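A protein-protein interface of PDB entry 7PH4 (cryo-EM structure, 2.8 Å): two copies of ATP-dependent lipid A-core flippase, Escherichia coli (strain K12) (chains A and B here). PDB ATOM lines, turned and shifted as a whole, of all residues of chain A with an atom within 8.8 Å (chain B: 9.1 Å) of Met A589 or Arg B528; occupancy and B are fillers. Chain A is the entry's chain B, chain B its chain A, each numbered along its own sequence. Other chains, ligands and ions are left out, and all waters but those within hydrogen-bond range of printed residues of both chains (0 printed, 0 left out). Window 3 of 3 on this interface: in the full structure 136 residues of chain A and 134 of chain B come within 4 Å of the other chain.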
ATOM      1  N   ARG A 388     -32.342  31.184   8.043  1.00  0.00           N
ATOM      2  CA  ARG A 388     -31.896  31.354   9.441  1.00  0.00           C
ATOM      3  C   ARG A 388     -33.123  31.514  10.331  1.00  0.00           C
ATOM      4  O   ARG A 388     -34.221  31.748   9.824  1.00  0.00           O
ATOM      5  CB  ARG A 388     -31.008  32.595   9.563  1.00  0.00           C
ATOM      6  CG  ARG A 388     -29.573  32.384   9.105  1.00  0.00           C
ATOM      7  CD  ARG A 388     -28.649  33.428   9.700  1.00  0.00           C
ATOM      8  NE  ARG A 388     -27.669  32.875  10.624  1.00  0.00           N
ATOM      9  CZ  ARG A 388     -27.730  32.989  11.947  1.00  0.00           C
ATOM     10  NH1 ARG A 388     -26.785  32.455  12.698  1.00  0.00           N
ATOM     11  NH2 ARG A 388     -28.734  33.636  12.512  1.00  0.00           N
ATOM     12  N   HIS A 548     -35.093  23.118   9.089  1.00  0.00           N
ATOM     13  CA  HIS A 548     -33.734  23.516   9.418  1.00  0.00           C
ATOM     14  C   HIS A 548     -32.709  22.446   9.092  1.00  0.00           C
ATOM     15  O   HIS A 548     -31.551  22.777   8.837  1.00  0.00           O
ATOM     16  CB  HIS A 548     -33.621  23.869  10.896  1.00  0.00           C
ATOM     17  CG  HIS A 548     -33.990  25.280  11.205  1.00  0.00           C
ATOM     18  ND1 HIS A 548     -33.516  26.347  10.480  1.00  0.00           N
ATOM     19  CD2 HIS A 548     -34.779  25.801  12.169  1.00  0.00           C
ATOM     20  CE1 HIS A 548     -34.000  27.466  10.983  1.00  0.00           C
ATOM     21  NE2 HIS A 548     -34.771  27.163  12.008  1.00  0.00           N
ATOM     22  N   LEU A 550     -31.393  20.069   6.402  1.00  0.00           N
ATOM     23  CA  LEU A 550     -31.523  19.959   4.960  1.00  0.00           C
ATOM     24  C   LEU A 550     -31.633  18.524   4.480  1.00  0.00           C
ATOM     25  O   LEU A 550     -31.902  18.310   3.297  1.00  0.00           O
ATOM     26  CB  LEU A 550     -30.344  20.636   4.282  1.00  0.00           C
ATOM     27  CG  LEU A 550     -30.055  22.047   4.768  1.00  0.00           C
ATOM     28  CD1 LEU A 550     -29.018  22.669   3.885  1.00  0.00           C
ATOM     29  CD2 LEU A 550     -31.307  22.876   4.775  1.00  0.00           C
ATOM     30  N   VAL A 582     -26.275  30.971  -1.063  1.00  0.00           N
ATOM     31  CA  VAL A 582     -26.531  30.770   0.359  1.00  0.00           C
ATOM     32  C   VAL A 582     -26.735  29.298   0.656  1.00  0.00           C
ATOM     33  O   VAL A 582     -26.219  28.770   1.647  1.00  0.00           O
ATOM     34  CB  VAL A 582     -27.754  31.588   0.804  1.00  0.00           C
ATOM     35  CG1 VAL A 582     -28.077  31.304   2.241  1.00  0.00           C
ATOM     36  CG2 VAL A 582     -27.512  33.038   0.623  1.00  0.00           C
ATOM     37  N   TYR A 583     -27.508  28.615  -0.179  1.00  0.00           N
ATOM     38  CA  TYR A 583     -27.840  27.231   0.111  1.00  0.00           C
ATOM     39  C   TYR A 583     -26.612  26.344   0.048  1.00  0.00           C
ATOM     40  O   TYR A 583     -26.506  25.379   0.805  1.00  0.00           O
ATOM     41  CB  TYR A 583     -28.907  26.728  -0.846  1.00  0.00           C
ATOM     42  CG  TYR A 583     -29.254  25.284  -0.639  1.00  0.00           C
ATOM     43  CD1 TYR A 583     -30.158  24.905   0.323  1.00  0.00           C
ATOM     44  CD2 TYR A 583     -28.674  24.303  -1.407  1.00  0.00           C
ATOM     45  CE1 TYR A 583     -30.472  23.597   0.511  1.00  0.00           C
ATOM     46  CE2 TYR A 583     -28.980  22.994  -1.223  1.00  0.00           C
ATOM     47  CZ  TYR A 583     -29.880  22.645  -0.266  1.00  0.00           C
ATOM     48  OH  TYR A 583     -30.190  21.323  -0.084  1.00  0.00           O
ATOM     49  N   ALA A 584     -25.682  26.632  -0.853  1.00  0.00           N
ATOM     50  CA  ALA A 584     -24.453  25.853  -0.872  1.00  0.00           C
ATOM     51  C   ALA A 584     -23.690  26.025   0.426  1.00  0.00           C
ATOM     52  O   ALA A 584     -23.087  25.076   0.929  1.00  0.00           O
ATOM     53  CB  ALA A 584     -23.589  26.248  -2.058  1.00  0.00           C
ATOM     54  N   GLN A 585     -23.716  27.224   0.993  1.00  0.00           N
ATOM     55  CA  GLN A 585     -23.059  27.451   2.270  1.00  0.00           C
ATOM     56  C   GLN A 585     -23.750  26.692   3.395  1.00  0.00           C
ATOM     57  O   GLN A 585     -23.085  26.071   4.233  1.00  0.00           O
ATOM     58  CB  GLN A 585     -23.020  28.943   2.565  1.00  0.00           C
ATOM     59  CG  GLN A 585     -22.037  29.315   3.637  1.00  0.00           C
ATOM     60  CD  GLN A 585     -20.638  28.832   3.329  1.00  0.00           C
ATOM     61  OE1 GLN A 585     -20.215  28.802   2.172  1.00  0.00           O
ATOM     62  NE2 GLN A 585     -19.908  28.445   4.366  1.00  0.00           N
ATOM     63  N   LEU A 586     -25.084  26.721   3.427  1.00  0.00           N
ATOM     64  CA  LEU A 586     -25.813  25.963   4.440  1.00  0.00           C
ATOM     65  C   LEU A 586     -25.534  24.476   4.317  1.00  0.00           C
ATOM     66  O   LEU A 586     -25.358  23.785   5.320  1.00  0.00           O
ATOM     67  CB  LEU A 586     -27.311  26.213   4.319  1.00  0.00           C
ATOM     68  CG  LEU A 586     -27.819  27.632   4.487  1.00  0.00           C
ATOM     69  CD1 LEU A 586     -29.293  27.687   4.189  1.00  0.00           C
ATOM     70  CD2 LEU A 586     -27.553  28.107   5.884  1.00  0.00           C
ATOM     71  N   HIS A 587     -25.515  23.965   3.095  1.00  0.00           N
ATOM     72  CA  HIS A 587     -25.236  22.556   2.876  1.00  0.00           C
ATOM     73  C   HIS A 587     -23.818  22.208   3.292  1.00  0.00           C
ATOM     74  O   HIS A 587     -23.579  21.149   3.875  1.00  0.00           O
ATOM     75  CB  HIS A 587     -25.469  22.222   1.412  1.00  0.00           C
ATOM     76  CG  HIS A 587     -25.378  20.769   1.098  1.00  0.00           C
ATOM     77  ND1 HIS A 587     -26.419  19.897   1.315  1.00  0.00           N
ATOM     78  CD2 HIS A 587     -24.375  20.035   0.567  1.00  0.00           C
ATOM     79  CE1 HIS A 587     -26.060  18.686   0.933  1.00  0.00           C
ATOM     80  NE2 HIS A 587     -24.824  18.742   0.477  1.00  0.00           N
ATOM     81  N   LYS A 588     -22.862  23.083   2.993  1.00  0.00           N
ATOM     82  CA  LYS A 588     -21.479  22.815   3.357  1.00  0.00           C
ATOM     83  C   LYS A 588     -21.303  22.762   4.864  1.00  0.00           C
ATOM     84  O   LYS A 588     -20.612  21.880   5.381  1.00  0.00           O
ATOM     85  CB  LYS A 588     -20.568  23.878   2.756  1.00  0.00           C
ATOM     86  CG  LYS A 588     -19.131  23.749   3.176  1.00  0.00           C
ATOM     87  CD  LYS A 588     -18.295  24.866   2.601  1.00  0.00           C
ATOM     88  CE  LYS A 588     -16.878  24.799   3.129  1.00  0.00           C
ATOM     89  NZ  LYS A 588     -16.264  23.469   2.868  1.00  0.00           N
ATOM     90  N   MET A 589     -21.928  23.677   5.589  1.00  0.00           N
ATOM     91  CA  MET A 589     -21.736  23.684   7.031  1.00  0.00           C
ATOM     92  C   MET A 589     -22.590  22.649   7.745  1.00  0.00           C
ATOM     93  O   MET A 589     -22.865  22.797   8.935  1.00  0.00           O
ATOM     94  CB  MET A 589     -21.992  25.081   7.597  1.00  0.00           C
ATOM     95  CG  MET A 589     -23.431  25.507   7.621  1.00  0.00           C
ATOM     96  SD  MET A 589     -23.587  27.221   8.134  1.00  0.00           S
ATOM     97  CE  MET A 589     -22.260  27.326   9.320  1.00  0.00           C
ATOM     98  N   GLN A 590     -23.010  21.600   7.054  1.00  0.00           N
ATOM     99  CA  GLN A 590     -23.899  20.620   7.642  1.00  0.00           C
ATOM    100  C   GLN A 590     -23.653  19.227   7.064  1.00  0.00           C
ATOM    101  O   GLN A 590     -22.979  19.040   6.054  1.00  0.00           O
ATOM    102  CB  GLN A 590     -25.339  21.056   7.414  1.00  0.00           C
ATOM    103  CG  GLN A 590     -26.365  20.342   8.235  1.00  0.00           C
ATOM    104  CD  GLN A 590     -27.704  21.031   8.189  1.00  0.00           C
ATOM    105  OE1 GLN A 590     -27.800  22.191   7.810  1.00  0.00           O
ATOM    106  NE2 GLN A 590     -28.747  20.322   8.576  1.00  0.00           N
ATOM    107  N   MET B 467     -24.099  35.791  25.028  1.00  0.00           N
ATOM    108  CA  MET B 467     -23.599  34.423  24.970  1.00  0.00           C
ATOM    109  C   MET B 467     -24.599  33.477  24.331  1.00  0.00           C
ATOM    110  O   MET B 467     -24.202  32.486  23.719  1.00  0.00           O
ATOM    111  CB  MET B 467     -23.243  33.925  26.361  1.00  0.00           C
ATOM    112  CG  MET B 467     -21.857  34.284  26.809  1.00  0.00           C
ATOM    113  SD  MET B 467     -21.385  33.280  28.223  1.00  0.00           S
ATOM    114  CE  MET B 467     -22.767  33.583  29.310  1.00  0.00           C
ATOM    115  N   TYR B 469     -26.402  34.229  21.853  1.00  0.00           N
ATOM    116  CA  TYR B 469     -26.572  34.681  20.481  1.00  0.00           C
ATOM    117  C   TYR B 469     -27.898  35.390  20.282  1.00  0.00           C
ATOM    118  O   TYR B 469     -28.400  35.472  19.167  1.00  0.00           O
ATOM    119  CB  TYR B 469     -26.434  33.515  19.507  1.00  0.00           C
ATOM    120  CG  TYR B 469     -26.087  33.910  18.105  1.00  0.00           C
ATOM    121  CD1 TYR B 469     -24.892  34.526  17.821  1.00  0.00           C
ATOM    122  CD2 TYR B 469     -26.943  33.643  17.062  1.00  0.00           C
ATOM    123  CE1 TYR B 469     -24.567  34.881  16.544  1.00  0.00           C
ATOM    124  CE2 TYR B 469     -26.627  33.992  15.781  1.00  0.00           C
ATOM    125  CZ  TYR B 469     -25.435  34.610  15.525  1.00  0.00           C
ATOM    126  OH  TYR B 469     -25.111  34.961  14.241  1.00  0.00           O
ATOM    127  N   THR B 519     -31.143  23.307  21.252  1.00  0.00           N
ATOM    128  CA  THR B 519     -30.886  23.877  19.943  1.00  0.00           C
ATOM    129  C   THR B 519     -31.705  23.172  18.882  1.00  0.00           C
ATOM    130  O   THR B 519     -31.232  22.918  17.776  1.00  0.00           O
ATOM    131  CB  THR B 519     -29.402  23.797  19.608  1.00  0.00           C
ATOM    132  OG1 THR B 519     -29.009  22.423  19.531  1.00  0.00           O
ATOM    133  CG2 THR B 519     -28.575  24.484  20.679  1.00  0.00           C
ATOM    134  N   LEU B 522     -33.008  25.962  16.290  1.00  0.00           N
ATOM    135  CA  LEU B 522     -31.965  26.826  15.772  1.00  0.00           C
ATOM    136  C   LEU B 522     -31.392  26.247  14.494  1.00  0.00           C
ATOM    137  O   LEU B 522     -31.338  25.033  14.315  1.00  0.00           O
ATOM    138  CB  LEU B 522     -30.852  26.993  16.794  1.00  0.00           C
ATOM    139  CG  LEU B 522     -31.270  27.510  18.157  1.00  0.00           C
ATOM    140  CD1 LEU B 522     -30.093  27.469  19.073  1.00  0.00           C
ATOM    141  CD2 LEU B 522     -31.768  28.910  18.006  1.00  0.00           C
ATOM    142  N   ASP B 523     -30.960  27.130  13.606  1.00  0.00           N
ATOM    143  CA  ASP B 523     -30.232  26.701  12.430  1.00  0.00           C
ATOM    144  C   ASP B 523     -28.813  26.322  12.830  1.00  0.00           C
ATOM    145  O   ASP B 523     -28.454  26.313  14.005  1.00  0.00           O
ATOM    146  CB  ASP B 523     -30.246  27.790  11.370  1.00  0.00           C
ATOM    147  CG  ASP B 523     -29.962  29.150  11.936  1.00  0.00           C
ATOM    148  OD1 ASP B 523     -30.590  29.520  12.941  1.00  0.00           O
ATOM    149  OD2 ASP B 523     -29.107  29.855  11.375  1.00  0.00           O
ATOM    150  N   THR B 524     -27.983  25.991  11.848  1.00  0.00           N
ATOM    151  CA  THR B 524     -26.666  25.473  12.185  1.00  0.00           C
ATOM    152  C   THR B 524     -25.711  26.577  12.611  1.00  0.00           C
ATOM    153  O   THR B 524     -24.950  26.395  13.561  1.00  0.00           O
ATOM    154  CB  THR B 524     -26.093  24.680  11.025  1.00  0.00           C
ATOM    155  OG1 THR B 524     -26.937  23.554  10.778  1.00  0.00           O
ATOM    156  CG2 THR B 524     -24.719  24.172  11.371  1.00  0.00           C
ATOM    157  N   GLU B 525     -25.718  27.722  11.933  1.00  0.00           N
ATOM    158  CA  GLU B 525     -24.776  28.767  12.323  1.00  0.00           C
ATOM    159  C   GLU B 525     -25.098  29.311  13.704  1.00  0.00           C
ATOM    160  O   GLU B 525     -24.193  29.565  14.506  1.00  0.00           O
ATOM    161  CB  GLU B 525     -24.763  29.897  11.304  1.00  0.00           C
ATOM    162  CG  GLU B 525     -23.586  30.828  11.502  1.00  0.00           C
ATOM    163  CD  GLU B 525     -23.551  31.966  10.509  1.00  0.00           C
ATOM    164  OE1 GLU B 525     -24.629  32.476  10.151  1.00  0.00           O
ATOM    165  OE2 GLU B 525     -22.444  32.354  10.081  1.00  0.00           O
ATOM    166  N   SER B 526     -26.379  29.491  14.002  1.00  0.00           N
ATOM    167  CA  SER B 526     -26.767  29.929  15.332  1.00  0.00           C
ATOM    168  C   SER B 526     -26.357  28.912  16.385  1.00  0.00           C
ATOM    169  O   SER B 526     -25.829  29.273  17.445  1.00  0.00           O
ATOM    170  CB  SER B 526     -28.269  30.166  15.366  1.00  0.00           C
ATOM    171  OG  SER B 526     -28.674  30.618  16.636  1.00  0.00           O
ATOM    172  N   GLU B 527     -26.581  27.633  16.102  1.00  0.00           N
ATOM    173  CA  GLU B 527     -26.201  26.581  17.035  1.00  0.00           C
ATOM    174  C   GLU B 527     -24.698  26.556  17.253  1.00  0.00           C
ATOM    175  O   GLU B 527     -24.232  26.332  18.372  1.00  0.00           O
ATOM    176  CB  GLU B 527     -26.702  25.237  16.519  1.00  0.00           C
ATOM    177  CG  GLU B 527     -28.195  25.090  16.503  1.00  0.00           C
ATOM    178  CD  GLU B 527     -28.642  23.766  15.915  1.00  0.00           C
ATOM    179  OE1 GLU B 527     -27.786  22.880  15.719  1.00  0.00           O
ATOM    180  OE2 GLU B 527     -29.853  23.609  15.660  1.00  0.00           O
ATOM    181  N   ARG B 528     -23.919  26.802  16.202  1.00  0.00           N
ATOM    182  CA  ARG B 528     -22.469  26.785  16.340  1.00  0.00           C
ATOM    183  C   ARG B 528     -21.970  27.982  17.129  1.00  0.00           C
ATOM    184  O   ARG B 528     -21.009  27.866  17.892  1.00  0.00           O
ATOM    185  CB  ARG B 528     -21.811  26.741  14.970  1.00  0.00           C
ATOM    186  CG  ARG B 528     -22.105  25.479  14.221  1.00  0.00           C
ATOM    187  CD  ARG B 528     -20.848  24.863  13.698  1.00  0.00           C
ATOM    188  NE  ARG B 528     -20.231  25.683  12.669  1.00  0.00           N
ATOM    189  CZ  ARG B 528     -20.047  25.280  11.421  1.00  0.00           C
ATOM    190  NH1 ARG B 528     -19.470  26.083  10.542  1.00  0.00           N
ATOM    191  NH2 ARG B 528     -20.428  24.066  11.057  1.00  0.00           N
ATOM    192  N   ALA B 529     -22.595  29.146  16.954  1.00  0.00           N
ATOM    193  CA  ALA B 529     -22.220  30.294  17.773  1.00  0.00           C
ATOM    194  C   ALA B 529     -22.512  30.037  19.245  1.00  0.00           C
ATOM    195  O   ALA B 529     -21.681  30.327  20.117  1.00  0.00           O
ATOM    196  CB  ALA B 529     -22.951  31.542  17.295  1.00  0.00           C
ATOM    197  N   ILE B 530     -23.682  29.478  19.543  1.00  0.00           N
ATOM    198  CA  ILE B 530     -24.004  29.156  20.928  1.00  0.00           C
ATOM    199  C   ILE B 530     -23.033  28.121  21.480  1.00  0.00           C
ATOM    200  O   ILE B 530     -22.610  28.204  22.635  1.00  0.00           O
ATOM    201  CB  ILE B 530     -25.461  28.689  21.037  1.00  0.00           C
ATOM    202  CG1 ILE B 530     -26.390  29.880  20.909  1.00  0.00           C
ATOM    203  CG2 ILE B 530     -25.699  28.007  22.341  1.00  0.00           C
ATOM    204  CD1 ILE B 530     -27.814  29.522  21.021  1.00  0.00           C
ATOM    205  N   GLN B 531     -22.661  27.135  20.667  1.00  0.00           N
ATOM    206  CA  GLN B 531     -21.705  26.127  21.114  1.00  0.00           C
ATOM    207  C   GLN B 531     -20.342  26.738  21.395  1.00  0.00           C
ATOM    208  O   GLN B 531     -19.659  26.341  22.342  1.00  0.00           O
ATOM    209  CB  GLN B 531     -21.582  25.026  20.071  1.00  0.00           C
ATOM    210  CG  GLN B 531     -20.619  23.939  20.451  1.00  0.00           C
ATOM    211  CD  GLN B 531     -21.069  23.199  21.677  1.00  0.00           C
ATOM    212  OE1 GLN B 531     -22.262  23.010  21.893  1.00  0.00           O
ATOM    213  NE2 GLN B 531     -20.118  22.779  22.499  1.00  0.00           N
ATOM    214  N   ALA B 532     -19.916  27.690  20.569  1.00  0.00           N
ATOM    215  CA  ALA B 532     -18.658  28.376  20.828  1.00  0.00           C
ATOM    216  C   ALA B 532     -18.707  29.129  22.147  1.00  0.00           C
ATOM    217  O   ALA B 532     -17.726  29.151  22.894  1.00  0.00           O
ATOM    218  CB  ALA B 532     -18.333  29.335  19.688  1.00  0.00           C
ATOM    219  N   ALA B 533     -19.834  29.772  22.442  1.00  0.00           N
ATOM    220  CA  ALA B 533     -19.950  30.451  23.730  1.00  0.00           C
ATOM    221  C   ALA B 533     -19.925  29.458  24.887  1.00  0.00           C
ATOM    222  O   ALA B 533     -19.288  29.707  25.918  1.00  0.00           O
ATOM    223  CB  ALA B 533     -21.223  31.287  23.769  1.00  0.00           C
ATOM    224  N   LEU B 534     -20.611  28.328  24.733  1.00  0.00           N
ATOM    225  CA  LEU B 534     -20.654  27.325  25.791  1.00  0.00           C
ATOM    226  C   LEU B 534     -19.280  26.738  26.060  1.00  0.00           C
ATOM    227  O   LEU B 534     -18.938  26.445  27.210  1.00  0.00           O
ATOM    228  CB  LEU B 534     -21.622  26.211  25.416  1.00  0.00           C
ATOM    229  CG  LEU B 534     -23.091  26.566  25.291  1.00  0.00           C
ATOM    230  CD1 LEU B 534     -23.854  25.387  24.778  1.00  0.00           C
ATOM    231  CD2 LEU B 534     -23.592  26.949  26.647  1.00  0.00           C
ATOM    232  N   ASP B 535     -18.489  26.527  25.013  1.00  0.00           N
ATOM    233  CA  ASP B 535     -17.180  25.913  25.196  1.00  0.00           C
ATOM    234  C   ASP B 535     -16.293  26.762  26.091  1.00  0.00           C
ATOM    235  O   ASP B 535     -15.607  26.241  26.974  1.00  0.00           O
ATOM    236  CB  ASP B 535     -16.516  25.683  23.843  1.00  0.00           C
ATOM    237  CG  ASP B 535     -17.138  24.535  23.079  1.00  0.00           C
ATOM    238  OD1 ASP B 535     -18.039  23.874  23.635  1.00  0.00           O
ATOM    239  OD2 ASP B 535     -16.730  24.290  21.926  1.00  0.00           O
ATOM    240  N   ARG B 549     -28.849  15.981  17.589  1.00  0.00           N
ATOM    241  CA  ARG B 549     -27.876  16.348  16.566  1.00  0.00           C
ATOM    242  C   ARG B 549     -26.504  16.053  17.093  1.00  0.00           C
ATOM    243  O   ARG B 549     -26.130  16.687  18.029  1.00  0.00           O
ATOM    244  CB  ARG B 549     -28.117  17.818  16.281  1.00  0.00           C
ATOM    245  CG  ARG B 549     -29.564  18.126  15.928  1.00  0.00           C
ATOM    246  CD  ARG B 549     -29.651  19.347  15.044  1.00  0.00           C
ATOM    247  NE  ARG B 549     -30.885  20.114  15.109  1.00  0.00           N
ATOM    248  CZ  ARG B 549     -31.031  21.274  14.477  1.00  0.00           C
ATOM    249  NH1 ARG B 549     -32.155  21.964  14.556  1.00  0.00           N
ATOM    250  NH2 ARG B 549     -30.026  21.756  13.773  1.00  0.00           N
ATOM    251  N   SER B 551     -23.690  16.762  15.909  1.00  0.00           N
ATOM    252  CA  SER B 551     -22.711  17.829  15.747  1.00  0.00           C
ATOM    253  C   SER B 551     -22.580  18.648  17.017  1.00  0.00           C
ATOM    254  O   SER B 551     -21.535  19.253  17.263  1.00  0.00           O
ATOM    255  CB  SER B 551     -23.100  18.723  14.579  1.00  0.00           C
ATOM    256  OG  SER B 551     -24.329  19.376  14.845  1.00  0.00           O
ATOM    257  N   THR B 552     -23.630  18.671  17.832  1.00  0.00           N
ATOM    258  CA  THR B 552     -23.622  19.460  19.052  1.00  0.00           C
ATOM    259  C   THR B 552     -22.739  18.843  20.128  1.00  0.00           C
ATOM    260  O   THR B 552     -22.195  19.562  20.970  1.00  0.00           O
ATOM    261  CB  THR B 552     -25.055  19.610  19.546  1.00  0.00           C
ATOM    262  OG1 THR B 552     -25.815  20.326  18.570  1.00  0.00           O
ATOM    263  CG2 THR B 552     -25.107  20.357  20.849  1.00  0.00           C
ATOM    264  N   LYS B 555     -17.662  17.052  21.107  1.00  0.00           N
ATOM    265  CA  LYS B 555     -16.570  17.319  22.029  1.00  0.00           C
ATOM    266  C   LYS B 555     -16.910  16.982  23.470  1.00  0.00           C
ATOM    267  O   LYS B 555     -16.151  17.340  24.371  1.00  0.00           O
ATOM    268  CB  LYS B 555     -16.141  18.777  21.925  1.00  0.00           C
ATOM    269  CG  LYS B 555     -15.328  19.064  20.690  1.00  0.00           C
ATOM    270  CD  LYS B 555     -14.923  20.513  20.618  1.00  0.00           C
ATOM    271  CE  LYS B 555     -13.979  20.732  19.457  1.00  0.00           C
ATOM    272  NZ  LYS B 555     -14.530  20.159  18.201  1.00  0.00           N
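NH1 of Arg A388 lies close to N of Ser B526. OH of Tyr B469 lies within hydrogen-bond range of NH1 of Arg A388 (3.4 Å). The guanidinium group (NE) of Arg A388 lies within salt-bridge range of the side-chain carboxylate (OD2) of Asp B523, 3.4 Å away. NH2 of Arg B528 lies within hydrogen-bond range of O of Met A589 (3.5 Å). The side-chain amide oxygen of Gln A590 lies within hydrogen-bond range of the side-chain hydroxyl of Thr B524 (3.4 Å). OE1 of Glu B525 is in salt-bridge range of NE of Arg A388, at 3.1 Å.
N of Leu A550 sits close to NE2 of Gln A590 (3.4 Å).
His A548 touches Asp B523. Met A589 touches Thr B524.
Of the printed residues of chain B, Arg A388 touches Tyr B469 (3.4 Å), Asp B523 (3.4 Å), Glu B525 (3.1 Å) and Ser B526 (3.3 Å). Printed residues of chain B within 4 Å of His A548: Asp B523 (3.7 Å). Of chain B, only Thr B524 and Arg B528 come within 4 Å of Met A589. Of the printed residues of chain A, Asp B523 touches Arg A388 (3.4 Å) and His A548 (3.7 Å). Printed residues of chain A within 4 Å of Glu B525: Arg A388 (3.1 Å). Of the printed residues of chain A, Ser B526 touches Arg A388 (3.3 Å). No residue of chain A comes within 4 Å of Ala B529. The nearest residue of chain A that does not touch Arg B528 is Gln A590 (5.4 Å).
Hydrophobic or aromatic side chains of chain A within 4 Å of the printed part of chain B: His A548 and Met A589. Of the 21 printed residues of chain B, 6 touch a printed residue of chain A. Printed residues of chain B that touch a printed residue of chain A: Tyr B469, Asp B523, Thr B524, Glu B525, Ser B526 and Arg B528. Hydrophobic or aromatic side chains of chain B within 4 Å of the printed part of chain A: Tyr B469. Among the printed residues, 8 pairs touch across the chains.
No position is printed for both chains. Of the 8 pairs that touch across the chains among the printed residues, none has its exchanged pair printed and touching as well.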
